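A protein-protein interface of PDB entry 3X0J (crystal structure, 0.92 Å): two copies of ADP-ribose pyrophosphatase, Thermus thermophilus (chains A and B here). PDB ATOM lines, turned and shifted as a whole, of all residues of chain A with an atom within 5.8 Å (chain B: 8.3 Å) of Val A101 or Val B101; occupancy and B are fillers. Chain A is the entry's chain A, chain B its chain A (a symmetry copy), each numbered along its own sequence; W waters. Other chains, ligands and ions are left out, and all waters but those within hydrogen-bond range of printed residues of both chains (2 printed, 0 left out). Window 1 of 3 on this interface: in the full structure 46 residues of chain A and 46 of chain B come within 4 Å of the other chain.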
ATOM      1  N   TYR A  99      22.574 -12.723  25.324  1.00  0.00           N
ATOM      2  CA  TYR A  99      21.593 -12.342  26.337  1.00  0.00           C
ATOM      3  C   TYR A  99      20.407 -13.270  26.291  1.00  0.00           C
ATOM      4  O   TYR A  99      20.030 -13.775  25.222  1.00  0.00           O
ATOM      5  CB  TYR A  99      21.145 -10.875  26.210  1.00  0.00           C
ATOM      6  CG  TYR A  99      20.361 -10.568  24.933  1.00  0.00           C
ATOM      7  CD1 TYR A  99      21.044 -10.237  23.747  1.00  0.00           C
ATOM      8  CD2 TYR A  99      18.990 -10.645  24.911  1.00  0.00           C
ATOM      9  CE1 TYR A  99      20.294  -9.979  22.577  1.00  0.00           C
ATOM     10  CE2 TYR A  99      18.252 -10.386  23.754  1.00  0.00           C
ATOM     11  CZ  TYR A  99      18.922 -10.051  22.569  1.00  0.00           C
ATOM     12  OH  TYR A  99      18.263  -9.810  21.415  1.00  0.00           O
ATOM     13  N   PHE A 100      19.792 -13.440  27.436  1.00  0.00           N
ATOM     14  CA  PHE A 100      18.492 -14.120  27.522  1.00  0.00           C
ATOM     15  C   PHE A 100      17.388 -13.104  27.300  1.00  0.00           C
ATOM     16  O   PHE A 100      17.309 -12.079  27.981  1.00  0.00           O
ATOM     17  CB  PHE A 100      18.322 -14.759  28.936  1.00  0.00           C
ATOM     18  CG  PHE A 100      19.215 -15.963  29.102  1.00  0.00           C
ATOM     19  CD1 PHE A 100      20.350 -15.917  29.893  1.00  0.00           C
ATOM     20  CD2 PHE A 100      18.920 -17.144  28.473  1.00  0.00           C
ATOM     21  CE1 PHE A 100      21.132 -17.086  30.097  1.00  0.00           C
ATOM     22  CE2 PHE A 100      19.704 -18.270  28.651  1.00  0.00           C
ATOM     23  CZ  PHE A 100      20.816 -18.224  29.386  1.00  0.00           C
ATOM     24  N   VAL A 101      16.510 -13.367  26.321  1.00  0.00           N
ATOM     25  CA  VAL A 101      15.537 -12.378  25.911  1.00  0.00           C
ATOM     26  C   VAL A 101      14.565 -11.985  27.014  1.00  0.00           C
ATOM     27  O   VAL A 101      14.128 -10.833  27.060  1.00  0.00           O
ATOM     28  CB  VAL A 101      14.754 -12.794  24.643  1.00  0.00           C
ATOM     29  CG1 VAL A 101      15.705 -13.277  23.532  1.00  0.00           C
ATOM     30  CG2 VAL A 101      13.681 -13.850  24.914  1.00  0.00           C
ATOM     31  N   SER A 102      14.177 -12.961  27.851  1.00  0.00           N
ATOM     32  CA  SER A 102      13.176 -12.724  28.909  1.00  0.00           C
ATOM     33  C   SER A 102      13.212 -13.900  29.849  1.00  0.00           C
ATOM     34  O   SER A 102      12.375 -14.810  29.782  1.00  0.00           O
ATOM     35  CB  SER A 102      11.784 -12.540  28.298  1.00  0.00           C
ATOM     36  OG  SER A 102      10.899 -12.124  29.335  1.00  0.00           O
ATOM     37  N   PRO A 103      14.224 -13.945  30.717  1.00  0.00           N
ATOM     38  CA  PRO A 103      14.473 -15.176  31.494  1.00  0.00           C
ATOM     39  C   PRO A 103      13.419 -15.421  32.582  1.00  0.00           C
ATOM     40  O   PRO A 103      13.470 -16.487  33.203  1.00  0.00           O
ATOM     41  CB  PRO A 103      15.865 -14.951  32.069  1.00  0.00           C
ATOM     42  CG  PRO A 103      15.954 -13.419  32.209  1.00  0.00           C
ATOM     43  CD  PRO A 103      15.238 -12.902  30.958  1.00  0.00           C
ATOM     44  N   PHE A 105      10.469 -16.108  31.796  1.00  0.00           N
ATOM     45  CA  PHE A 105       9.561 -17.123  31.265  1.00  0.00           C
ATOM     46  C   PHE A 105      10.139 -17.964  30.148  1.00  0.00           C
ATOM     47  O   PHE A 105       9.551 -19.032  29.909  1.00  0.00           O
ATOM     48  CB  PHE A 105       8.185 -16.549  30.860  1.00  0.00           C
ATOM     49  CG  PHE A 105       8.168 -16.012  29.432  1.00  0.00           C
ATOM     50  CD1 PHE A 105       7.623 -16.799  28.418  1.00  0.00           C
ATOM     51  CD2 PHE A 105       8.680 -14.755  29.133  1.00  0.00           C
ATOM     52  CE1 PHE A 105       7.571 -16.329  27.109  1.00  0.00           C
ATOM     53  CE2 PHE A 105       8.621 -14.304  27.775  1.00  0.00           C
ATOM     54  CZ  PHE A 105       8.039 -15.073  26.783  1.00  0.00           C
ATOM     55  N   THR A 106      11.181 -17.560  29.459  1.00  0.00           N
ATOM     56  CA  THR A 106      11.696 -18.362  28.364  1.00  0.00           C
ATOM     57  C   THR A 106      13.180 -18.530  28.498  1.00  0.00           C
ATOM     58  O   THR A 106      13.883 -17.706  29.096  1.00  0.00           O
ATOM     59  CB  THR A 106      11.309 -17.738  26.969  1.00  0.00           C
ATOM     60  OG1 THR A 106      11.785 -18.593  25.922  1.00  0.00           O
ATOM     61  CG2 THR A 106      11.907 -16.369  26.740  1.00  0.00           C
ATOM     62  N   GLU A 108      15.033 -18.614  25.680  1.00  0.00           N
ATOM     63  CA  GLU A 108      15.658 -18.136  24.441  1.00  0.00           C
ATOM     64  C   GLU A 108      16.896 -17.301  24.790  1.00  0.00           C
ATOM     65  O   GLU A 108      16.803 -16.325  25.534  1.00  0.00           O
ATOM     66  CB  GLU A 108      14.692 -17.294  23.617  1.00  0.00           C
ATOM     67  CG  GLU A 108      15.337 -16.857  22.289  1.00  0.00           C
ATOM     68  CD  GLU A 108      14.406 -16.016  21.429  1.00  0.00           C
ATOM     69  OE1 GLU A 108      13.282 -15.725  21.821  1.00  0.00           O
ATOM     70  OE2 GLU A 108      14.933 -15.630  20.302  1.00  0.00           O
ATOM     71  N   LYS A 109      18.019 -17.669  24.191  1.00  0.00           N
ATOM     72  CA  LYS A 109      19.289 -17.004  24.349  1.00  0.00           C
ATOM     73  C   LYS A 109      19.742 -16.538  22.956  1.00  0.00           C
ATOM     74  O   LYS A 109      19.722 -17.333  22.033  1.00  0.00           O
ATOM     75  CB  LYS A 109      20.309 -17.951  24.938  1.00  0.00           C
ATOM     76  CG  LYS A 109      21.592 -17.282  25.398  1.00  0.00           C
ATOM     77  CD  LYS A 109      22.574 -18.280  25.976  1.00  0.00           C
ATOM     78  CE  LYS A 109      23.693 -17.577  26.697  1.00  0.00           C
ATOM     79  NZ  LYS A 109      24.644 -18.553  27.296  1.00  0.00           N
ATOM     80  N   THR A 110      20.152 -15.283  22.870  1.00  0.00           N
ATOM     81  CA  THR A 110      20.554 -14.672  21.614  1.00  0.00           C
ATOM     82  C   THR A 110      22.045 -14.369  21.648  1.00  0.00           C
ATOM     83  O   THR A 110      22.529 -13.710  22.556  1.00  0.00           O
ATOM     84  CB  THR A 110      19.764 -13.383  21.384  1.00  0.00           C
ATOM     85  OG1 THR A 110      18.380 -13.694  21.486  1.00  0.00           O
ATOM     86  CG2 THR A 110      20.051 -12.774  20.031  1.00  0.00           C
ATOM     87  N   SER A 153      12.775  -4.227  18.058  1.00  0.00           N
ATOM     88  CA  SER A 153      13.003  -5.473  18.778  1.00  0.00           C
ATOM     89  C   SER A 153      14.203  -5.297  19.713  1.00  0.00           C
ATOM     90  O   SER A 153      14.991  -4.369  19.569  1.00  0.00           O
ATOM     91  CB  SER A 153      13.281  -6.619  17.814  1.00  0.00           C
ATOM     92  OG  SER A 153      14.534  -6.360  17.159  1.00  0.00           O
ATOM     93  N   ALA A 154      14.393  -6.270  20.609  1.00  0.00           N
ATOM     94  CA  ALA A 154      15.602  -6.264  21.421  1.00  0.00           C
ATOM     95  C   ALA A 154      16.829  -6.215  20.527  1.00  0.00           C
ATOM     96  O   ALA A 154      17.785  -5.489  20.828  1.00  0.00           O
ATOM     97  CB  ALA A 154      15.659  -7.494  22.310  1.00  0.00           C
ATOM     98  N   THR A 155      16.842  -6.994  19.436  1.00  0.00           N
ATOM     99  CA  THR A 155      18.044  -7.002  18.619  1.00  0.00           C
ATOM    100  C   THR A 155      18.293  -5.655  17.976  1.00  0.00           C
ATOM    101  O   THR A 155      19.450  -5.211  17.884  1.00  0.00           O
ATOM    102  CB  THR A 155      18.007  -8.137  17.552  1.00  0.00           C
ATOM    103  OG1 THR A 155      16.883  -7.912  16.682  1.00  0.00           O
ATOM    104  CG2 THR A 155      17.957  -9.512  18.196  1.00  0.00           C
ATOM    105  N   VAL B  31       2.946 -16.387  22.059  1.00  0.00           N
ATOM    106  CA  VAL B  31       2.859 -16.278  23.503  1.00  0.00           C
ATOM    107  C   VAL B  31       2.498 -14.853  23.863  1.00  0.00           C
ATOM    108  O   VAL B  31       3.308 -13.913  23.665  1.00  0.00           O
ATOM    109  CB  VAL B  31       4.123 -16.732  24.169  1.00  0.00           C
ATOM    110  CG1 VAL B  31       4.027 -16.506  25.697  1.00  0.00           C
ATOM    111  CG2 VAL B  31       4.387 -18.221  23.880  1.00  0.00           C
ATOM    112  N   HIS B  33       1.977 -12.014  26.578  1.00  0.00           N
ATOM    113  CA  HIS B  33       2.649 -11.829  27.864  1.00  0.00           C
ATOM    114  C   HIS B  33       2.438 -10.381  28.262  1.00  0.00           C
ATOM    115  O   HIS B  33       2.429  -9.470  27.444  1.00  0.00           O
ATOM    116  CB  HIS B  33       4.135 -12.121  27.619  1.00  0.00           C
ATOM    117  CG  HIS B  33       5.025 -12.100  28.847  1.00  0.00           C
ATOM    118  ND1 HIS B  33       5.351 -10.935  29.558  1.00  0.00           N
ATOM    119  CD2 HIS B  33       5.695 -13.088  29.442  1.00  0.00           C
ATOM    120  CE1 HIS B  33       6.212 -11.268  30.517  1.00  0.00           C
ATOM    121  NE2 HIS B  33       6.425 -12.571  30.490  1.00  0.00           N
ATOM    122  N   LYS B  34       2.338 -10.142  29.591  1.00  0.00           N
ATOM    123  CA  LYS B  34       2.161  -8.768  30.023  1.00  0.00           C
ATOM    124  C   LYS B  34       3.380  -7.924  29.620  1.00  0.00           C
ATOM    125  O   LYS B  34       4.496  -8.416  29.541  1.00  0.00           O
ATOM    126  CB  LYS B  34       2.058  -8.680  31.575  1.00  0.00           C
ATOM    127  CG  LYS B  34       0.659  -9.149  32.050  1.00  0.00           C
ATOM    128  CD  LYS B  34       0.505  -8.760  33.529  1.00  0.00           C
ATOM    129  CE  LYS B  34      -0.922  -8.912  34.012  1.00  0.00           C
ATOM    130  NZ  LYS B  34      -1.397 -10.265  33.583  1.00  0.00           N
ATOM    131  N   PRO B  35       3.157  -6.628  29.446  1.00  0.00           N
ATOM    132  CA  PRO B  35       4.293  -5.734  29.264  1.00  0.00           C
ATOM    133  C   PRO B  35       5.076  -5.579  30.520  1.00  0.00           C
ATOM    134  O   PRO B  35       4.608  -5.863  31.621  1.00  0.00           O
ATOM    135  CB  PRO B  35       3.652  -4.406  28.786  1.00  0.00           C
ATOM    136  CG  PRO B  35       2.252  -4.426  29.251  1.00  0.00           C
ATOM    137  CD  PRO B  35       1.857  -5.852  29.420  1.00  0.00           C
ATOM    138  N   ALA B  36       6.320  -5.104  30.334  1.00  0.00           N
ATOM    139  CA  ALA B  36       7.308  -5.057  31.393  1.00  0.00           C
ATOM    140  C   ALA B  36       7.974  -3.675  31.423  1.00  0.00           C
ATOM    141  O   ALA B  36       7.895  -2.905  30.479  1.00  0.00           O
ATOM    142  CB  ALA B  36       8.362  -6.156  31.194  1.00  0.00           C
ATOM    143  N   VAL B  57      15.743 -20.615  32.926  1.00  0.00           N
ATOM    144  CA  VAL B  57      17.092 -20.812  32.401  1.00  0.00           C
ATOM    145  C   VAL B  57      18.031 -21.556  33.339  1.00  0.00           C
ATOM    146  O   VAL B  57      19.150 -21.928  32.950  1.00  0.00           O
ATOM    147  CB  VAL B  57      17.778 -19.475  31.986  1.00  0.00           C
ATOM    148  CG1 VAL B  57      16.952 -18.912  30.841  1.00  0.00           C
ATOM    149  CG2 VAL B  57      17.825 -18.485  33.081  1.00  0.00           C
ATOM    150  N   GLU B  63      20.650  -8.865  35.587  1.00  0.00           N
ATOM    151  CA  GLU B  63      19.527  -8.075  35.094  1.00  0.00           C
ATOM    152  C   GLU B  63      19.624  -6.693  35.714  1.00  0.00           C
ATOM    153  O   GLU B  63      20.476  -6.430  36.553  1.00  0.00           O
ATOM    154  CB  GLU B  63      18.198  -8.737  35.454  1.00  0.00           C
ATOM    155  CG  GLU B  63      18.168 -10.215  35.145  1.00  0.00           C
ATOM    156  CD  GLU B  63      16.818 -10.874  35.252  1.00  0.00           C
ATOM    157  OE1 GLU B  63      15.743 -10.160  35.108  1.00  0.00           O
ATOM    158  OE2 GLU B  63      16.762 -12.105  35.451  1.00  0.00           O
ATOM    159  N   SER B  98      11.681   1.691  24.336  1.00  0.00           N
ATOM    160  CA  SER B  98      11.034   0.392  24.555  1.00  0.00           C
ATOM    161  C   SER B  98      11.503  -0.588  23.517  1.00  0.00           C
ATOM    162  O   SER B  98      12.030  -0.245  22.463  1.00  0.00           O
ATOM    163  CB  SER B  98       9.499   0.521  24.445  1.00  0.00           C
ATOM    164  OG  SER B  98       9.141   0.853  23.120  1.00  0.00           O
ATOM    165  N   TYR B  99      11.267  -1.882  23.802  1.00  0.00           N
ATOM    166  CA  TYR B  99      11.610  -2.922  22.836  1.00  0.00           C
ATOM    167  C   TYR B  99      10.729  -4.128  23.032  1.00  0.00           C
ATOM    168  O   TYR B  99      10.314  -4.442  24.159  1.00  0.00           O
ATOM    169  CB  TYR B  99      13.097  -3.316  22.887  1.00  0.00           C
ATOM    170  CG  TYR B  99      13.520  -3.996  24.190  1.00  0.00           C
ATOM    171  CD1 TYR B  99      13.910  -3.220  25.298  1.00  0.00           C
ATOM    172  CD2 TYR B  99      13.492  -5.363  24.313  1.00  0.00           C
ATOM    173  CE1 TYR B  99      14.275  -3.875  26.496  1.00  0.00           C
ATOM    174  CE2 TYR B  99      13.857  -6.008  25.497  1.00  0.00           C
ATOM    175  CZ  TYR B  99      14.251  -5.245  26.606  1.00  0.00           C
ATOM    176  OH  TYR B  99      14.595  -5.810  27.782  1.00  0.00           O
ATOM    177  N   PHE B 100      10.501  -4.830  21.948  1.00  0.00           N
ATOM    178  CA  PHE B 100       9.862  -6.153  22.003  1.00  0.00           C
ATOM    179  C   PHE B 100      10.929  -7.206  22.228  1.00  0.00           C
ATOM    180  O   PHE B 100      11.905  -7.304  21.482  1.00  0.00           O
ATOM    181  CB  PHE B 100       9.131  -6.443  20.655  1.00  0.00           C
ATOM    182  CG  PHE B 100       7.889  -5.600  20.514  1.00  0.00           C
ATOM    183  CD1 PHE B 100       7.840  -4.525  19.645  1.00  0.00           C
ATOM    184  CD2 PHE B 100       6.765  -5.884  21.246  1.00  0.00           C
ATOM    185  CE1 PHE B 100       6.632  -3.795  19.471  1.00  0.00           C
ATOM    186  CE2 PHE B 100       5.604  -5.149  21.096  1.00  0.00           C
ATOM    187  CZ  PHE B 100       5.559  -4.092  20.283  1.00  0.00           C
ATOM    188  N   VAL B 101      10.765  -8.019  23.283  1.00  0.00           N
ATOM    189  CA  VAL B 101      11.814  -8.930  23.687  1.00  0.00           C
ATOM    190  C   VAL B 101      12.162  -9.967  22.630  1.00  0.00           C
ATOM    191  O   VAL B 101      13.322 -10.372  22.531  1.00  0.00           O
ATOM    192  CB  VAL B 101      11.515  -9.631  25.034  1.00  0.00           C
ATOM    193  CG1 VAL B 101      11.079  -8.617  26.108  1.00  0.00           C
ATOM    194  CG2 VAL B 101      10.480 -10.751  24.917  1.00  0.00           C
ATOM    195  N   SER B 102      11.144 -10.444  21.895  1.00  0.00           N
ATOM    196  CA  SER B 102      11.341 -11.511  20.896  1.00  0.00           C
ATOM    197  C   SER B 102      10.102 -11.579  20.044  1.00  0.00           C
ATOM    198  O   SER B 102       9.227 -12.435  20.235  1.00  0.00           O
ATOM    199  CB  SER B 102      11.616 -12.849  21.588  1.00  0.00           C
ATOM    200  OG  SER B 102      11.988 -13.794  20.588  1.00  0.00           O
ATOM    201  N   PRO B 103       9.960 -10.634  19.112  1.00  0.00           N
ATOM    202  CA  PRO B 103       8.670 -10.478  18.410  1.00  0.00           C
ATOM    203  C   PRO B 103       8.385 -11.615  17.420  1.00  0.00           C
ATOM    204  O   PRO B 103       7.278 -11.640  16.875  1.00  0.00           O
ATOM    205  CB  PRO B 103       8.805  -9.126  17.725  1.00  0.00           C
ATOM    206  CG  PRO B 103      10.320  -9.001  17.468  1.00  0.00           C
ATOM    207  CD  PRO B 103      10.948  -9.610  18.725  1.00  0.00           C
ATOM    208  N   GLY B 104       9.335 -12.542  17.209  1.00  0.00           N
ATOM    209  CA  GLY B 104       9.028 -13.725  16.444  1.00  0.00           C
ATOM    210  C   GLY B 104       8.090 -14.689  17.160  1.00  0.00           C
ATOM    211  O   GLY B 104       7.541 -15.574  16.493  1.00  0.00           O
ATOM    212  N   PHE B 105       7.858 -14.519  18.459  1.00  0.00           N
ATOM    213  CA  PHE B 105       6.915 -15.416  19.124  1.00  0.00           C
ATOM    214  C   PHE B 105       6.134 -14.784  20.257  1.00  0.00           C
ATOM    215  O   PHE B 105       5.107 -15.385  20.613  1.00  0.00           O
ATOM    216  CB  PHE B 105       7.563 -16.742  19.582  1.00  0.00           C
ATOM    217  CG  PHE B 105       8.199 -16.640  20.965  1.00  0.00           C
ATOM    218  CD1 PHE B 105       7.505 -17.132  22.070  1.00  0.00           C
ATOM    219  CD2 PHE B 105       9.456 -16.069  21.136  1.00  0.00           C
ATOM    220  CE1 PHE B 105       8.067 -17.075  23.342  1.00  0.00           C
ATOM    221  CE2 PHE B 105      10.003 -16.017  22.458  1.00  0.00           C
ATOM    222  CZ  PHE B 105       9.326 -16.547  23.542  1.00  0.00           C
ATOM    223  N   THR B 106       6.549 -13.683  20.839  1.00  0.00           N
ATOM    224  CA  THR B 106       5.809 -13.113  21.951  1.00  0.00           C
ATOM    225  C   THR B 106       5.581 -11.649  21.725  1.00  0.00           C
ATOM    226  O   THR B 106       6.336 -10.968  21.021  1.00  0.00           O
ATOM    227  CB  THR B 106       6.543 -13.380  23.320  1.00  0.00           C
ATOM    228  OG1 THR B 106       5.748 -12.855  24.391  1.00  0.00           O
ATOM    229  CG2 THR B 106       7.904 -12.727  23.407  1.00  0.00           C
ATOM    230  N   ASP B 107       4.524 -11.116  22.387  1.00  0.00           N
ATOM    231  CA  ASP B 107       4.244  -9.714  22.360  1.00  0.00           C
ATOM    232  C   ASP B 107       4.794  -8.983  23.578  1.00  0.00           C
ATOM    233  O   ASP B 107       4.503  -7.771  23.701  1.00  0.00           O
ATOM    234  CB  ASP B 107       2.760  -9.389  22.187  1.00  0.00           C
ATOM    235  CG  ASP B 107       1.960  -9.961  23.367  1.00  0.00           C
ATOM    236  OD1 ASP B 107       0.718  -9.806  23.274  1.00  0.00           O
ATOM    237  OD2 ASP B 107       2.505 -10.490  24.311  1.00  0.00           O
ATOM    238  N   GLU B 108       5.631  -9.600  24.404  1.00  0.00           N
ATOM    239  CA  GLU B 108       6.173  -8.873  25.559  1.00  0.00           C
ATOM    240  C   GLU B 108       6.938  -7.639  25.064  1.00  0.00           C
ATOM    241  O   GLU B 108       7.862  -7.757  24.260  1.00  0.00           O
ATOM    242  CB  GLU B 108       7.104  -9.751  26.385  1.00  0.00           C
ATOM    243  CG  GLU B 108       7.610  -9.000  27.629  1.00  0.00           C
ATOM    244  CD  GLU B 108       8.542  -9.839  28.489  1.00  0.00           C
ATOM    245  OE1 GLU B 108       8.844 -10.981  28.158  1.00  0.00           O
ATOM    246  OE2 GLU B 108       8.987  -9.221  29.546  1.00  0.00           O
ATOM    247  N   LYS B 109       6.574  -6.487  25.608  1.00  0.00           N
ATOM    248  CA  LYS B 109       7.182  -5.213  25.314  1.00  0.00           C
ATOM    249  C   LYS B 109       7.729  -4.646  26.634  1.00  0.00           C
ATOM    250  O   LYS B 109       7.002  -4.623  27.610  1.00  0.00           O
ATOM    251  CB  LYS B 109       6.160  -4.267  24.724  1.00  0.00           C
ATOM    252  CG  LYS B 109       6.752  -3.001  24.128  1.00  0.00           C
ATOM    253  CD  LYS B 109       5.682  -2.093  23.556  1.00  0.00           C
ATOM    254  CE  LYS B 109       6.293  -1.009  22.709  1.00  0.00           C
ATOM    255  NZ  LYS B 109       5.246  -0.134  22.118  1.00  0.00           N
ATOM    256  N   THR B 110       8.971  -4.194  26.599  1.00  0.00           N
ATOM    257  CA  THR B 110       9.656  -3.684  27.777  1.00  0.00           C
ATOM    258  C   THR B 110       9.903  -2.192  27.616  1.00  0.00           C
ATOM    259  O   THR B 110      10.479  -1.756  26.631  1.00  0.00           O
ATOM    260  CB  THR B 110      10.983  -4.417  27.967  1.00  0.00           C
ATOM    261  OG1 THR B 110      10.714  -5.813  27.986  1.00  0.00           O
ATOM    262  CG2 THR B 110      11.676  -4.015  29.248  1.00  0.00           C
ATOM    263  N   HIS B 111       9.511  -1.426  28.643  1.00  0.00           N
ATOM    264  CA  HIS B 111       9.682   0.005  28.689  1.00  0.00           C
ATOM    265  C   HIS B 111      10.826   0.327  29.644  1.00  0.00           C
ATOM    266  O   HIS B 111      10.765  -0.057  30.815  1.00  0.00           O
ATOM    267  CB  HIS B 111       8.410   0.680  29.178  1.00  0.00           C
ATOM    268  CG  HIS B 111       7.222   0.318  28.330  1.00  0.00           C
ATOM    269  ND1 HIS B 111       6.847   1.024  27.280  1.00  0.00           N
ATOM    270  CD2 HIS B 111       6.359  -0.725  28.438  1.00  0.00           C
ATOM    271  CE1 HIS B 111       5.761   0.491  26.733  1.00  0.00           C
ATOM    272  NE2 HIS B 111       5.431  -0.569  27.436  1.00  0.00           N
ATOM    273  N   PHE B 152      23.828 -12.398  30.807  1.00  0.00           N
ATOM    274  CA  PHE B 152      22.969 -11.224  30.838  1.00  0.00           C
ATOM    275  C   PHE B 152      21.533 -11.583  30.508  1.00  0.00           C
ATOM    276  O   PHE B 152      21.310 -12.424  29.636  1.00  0.00           O
ATOM    277  CB  PHE B 152      23.397 -10.216  29.768  1.00  0.00           C
ATOM    278  CG  PHE B 152      24.591  -9.370  30.123  1.00  0.00           C
ATOM    279  CD1 PHE B 152      25.702  -9.319  29.260  1.00  0.00           C
ATOM    280  CD2 PHE B 152      24.551  -8.547  31.234  1.00  0.00           C
ATOM    281  CE1 PHE B 152      26.759  -8.486  29.584  1.00  0.00           C
ATOM    282  CE2 PHE B 152      25.642  -7.743  31.557  1.00  0.00           C
ATOM    283  CZ  PHE B 152      26.748  -7.686  30.724  1.00  0.00           C
ATOM    284  N   SER B 153      20.587 -10.873  31.103  1.00  0.00           N
ATOM    285  CA  SER B 153      19.286 -10.734  30.461  1.00  0.00           C
ATOM    286  C   SER B 153      19.355  -9.600  29.434  1.00  0.00           C
ATOM    287  O   SER B 153      20.263  -8.778  29.454  1.00  0.00           O
ATOM    288  CB  SER B 153      18.202 -10.420  31.483  1.00  0.00           C
ATOM    289  OG  SER B 153      18.463  -9.117  32.029  1.00  0.00           O
ATOM    290  N   ALA B 154      18.315  -9.505  28.600  1.00  0.00           N
ATOM    291  CA  ALA B 154      18.223  -8.359  27.706  1.00  0.00           C
ATOM    292  C   ALA B 154      18.291  -7.070  28.505  1.00  0.00           C
ATOM    293  O   ALA B 154      18.961  -6.117  28.087  1.00  0.00           O
ATOM    294  CB  ALA B 154      16.932  -8.403  26.907  1.00  0.00           C
ATOM    295  N   THR B 155      17.591  -6.999  29.647  1.00  0.00           N
ATOM    296  CA  THR B 155      17.598  -5.742  30.375  1.00  0.00           C
ATOM    297  C   THR B 155      18.978  -5.408  30.901  1.00  0.00           C
ATOM    298  O   THR B 155      19.387  -4.234  30.878  1.00  0.00           O
ATOM    299  CB  THR B 155      16.544  -5.735  31.522  1.00  0.00           C
ATOM    300  OG1 THR B 155      16.867  -6.786  32.451  1.00  0.00           O
ATOM    301  CG2 THR B 155      15.129  -5.873  30.985  1.00  0.00           C
HETATM  302  O   HOH W   1      15.645 -10.812  21.045  1.00  0.00           O
HETATM  303  O   HOH W   2      13.714  -8.422  28.407  1.00  0.00           O
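Tyr A99 touches Ala B154, and with the chains exchanged Ala A154 touches Tyr B99.
Pro A103 touches Ser B153, and with the chains exchanged Ser A153 touches Pro B103.
Phe A105 touches Glu B108, and with the chains exchanged Glu A108 touches Phe B105.
Positions printed for both chains: 99, 100, 101, 102, 103, 105, 106, 108, 109, 110, 153, 154 and 155.
Of the 27 pairs that touch across the chains among the printed residues, 20 have their exchanged pair printed and touching as well.
Water W2 lies within hydrogen-bond range of the backbone carbonyl oxygen (O) of Val A101 (2.8 Å) and the side-chain hydroxyl (OH) of Tyr B99 (2.8 Å).
Water W1 lies within hydrogen-bond range of the backbone carbonyl oxygen (O) of Val B101 and the side-chain hydroxyl (OH) of Tyr A99.
N of Phe A100 lies within hydrogen-bond range of O of Phe B152, 2.9 Å away.
The backbone carbonyl oxygen (O) of Phe A100 is in hydrogen-bond range of the backbone NH (N) of Ala B154.
The side-chain carboxylate (OE1) of Glu B108 sits at hydrogen-bond distance from the side-chain hydroxyl (OG) of Ser A102, 2.6 Å away.
The side-chain carboxylate (OE1) of Glu A108 is in hydrogen-bond range of the side-chain hydroxyl (OG) of Ser B102 (2.6 Å).
The backbone carbonyl oxygen (O) of Phe B100 lies within hydrogen-bond range of the backbone NH (N) of Ala A154, 2.8 Å away.
Of the printed residues of chain B, Ser A153 touches Tyr B99, Phe B100 and Pro B103.
Of the printed residues of chain A, Tyr B99 touches Ser A153 (3.9 Å) and Ala A154 (3.6 Å).
Val B101 touches two residues of chain A.
Of the printed residues of chain A, Ser B102 touches Glu A108 (2.6 Å).
Of the printed residues of chain A, Ala B154 touches Tyr A99 (3.6 Å), Phe A100 (2.8 Å) and Val A101 (3.7 Å).
The nearest residue of chain B that does not touch Val A101 is Ser B102 (4.04 Å).
The nearest residue of chain A that does not touch Val B101 is Ser A102 (4.04 Å).
Ser B153 touches Tyr A99 (C to CB, 3.9 Å).
CG of Pro A103 touches OE2 of Glu B63, at 3.6 Å.
Pro A103 touches Ser B153 (CG to CB, 3.8 Å).
Val B31 touches Phe A105.
Glu B108 touches Phe A105.
Thr A106 touches Val B57.
Thr A106 touches Phe B105 (OG1 to CZ, 3.99 Å).
Phe B105 touches Glu A108.
O of Phe B100 touches CA of Ser A153, at 3.4 Å.
Ala A154 touches Val B101 (CB to O, 3.7 Å).
Hydrophobic or aromatic side chains of chain B that line the printed part of chain A: Val B31, His B33, Val B57, Tyr B99, Val B101, Pro B103, Phe B105 and Ala B154.
Of the 13 printed residues of chain A, 10 touch a printed residue of chain B.
Printed residues of chain A that touch a printed residue of chain B: Tyr A99, Phe A100, Val A101, Ser A102, Pro A103, Phe A105, Thr A106, Glu A108, Ser A153 and Ala A154.
Among the printed residues, 27 pairs touch across the chains.
Among the printed residues, no Asp or Glu carboxylate lies within 4 Å of a Lys or Arg side-chain nitrogen of the other chain.
O of Tyr A99 is in hydrogen-bond range of N of Thr A110 (2.8 Å).
The backbone NH (N) of Glu A108 lies within hydrogen-bond range of the side-chain hydroxyl (OG1) of Thr A106, at 3.3 Å.
The side-chain hydroxyl of Ser A153 lies within hydrogen-bond range of the side-chain hydroxyl of Thr A155 (2.9 Å).
O of Val B31 sits at hydrogen-bond distance from OG1 of Thr B106 (2.8 Å).
N of Val B101 is in hydrogen-bond range of O of Glu B108.
The side-chain hydroxyl of Thr B155 lies within hydrogen-bond range of the side-chain hydroxyl of Ser B153, 2.9 Å away.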
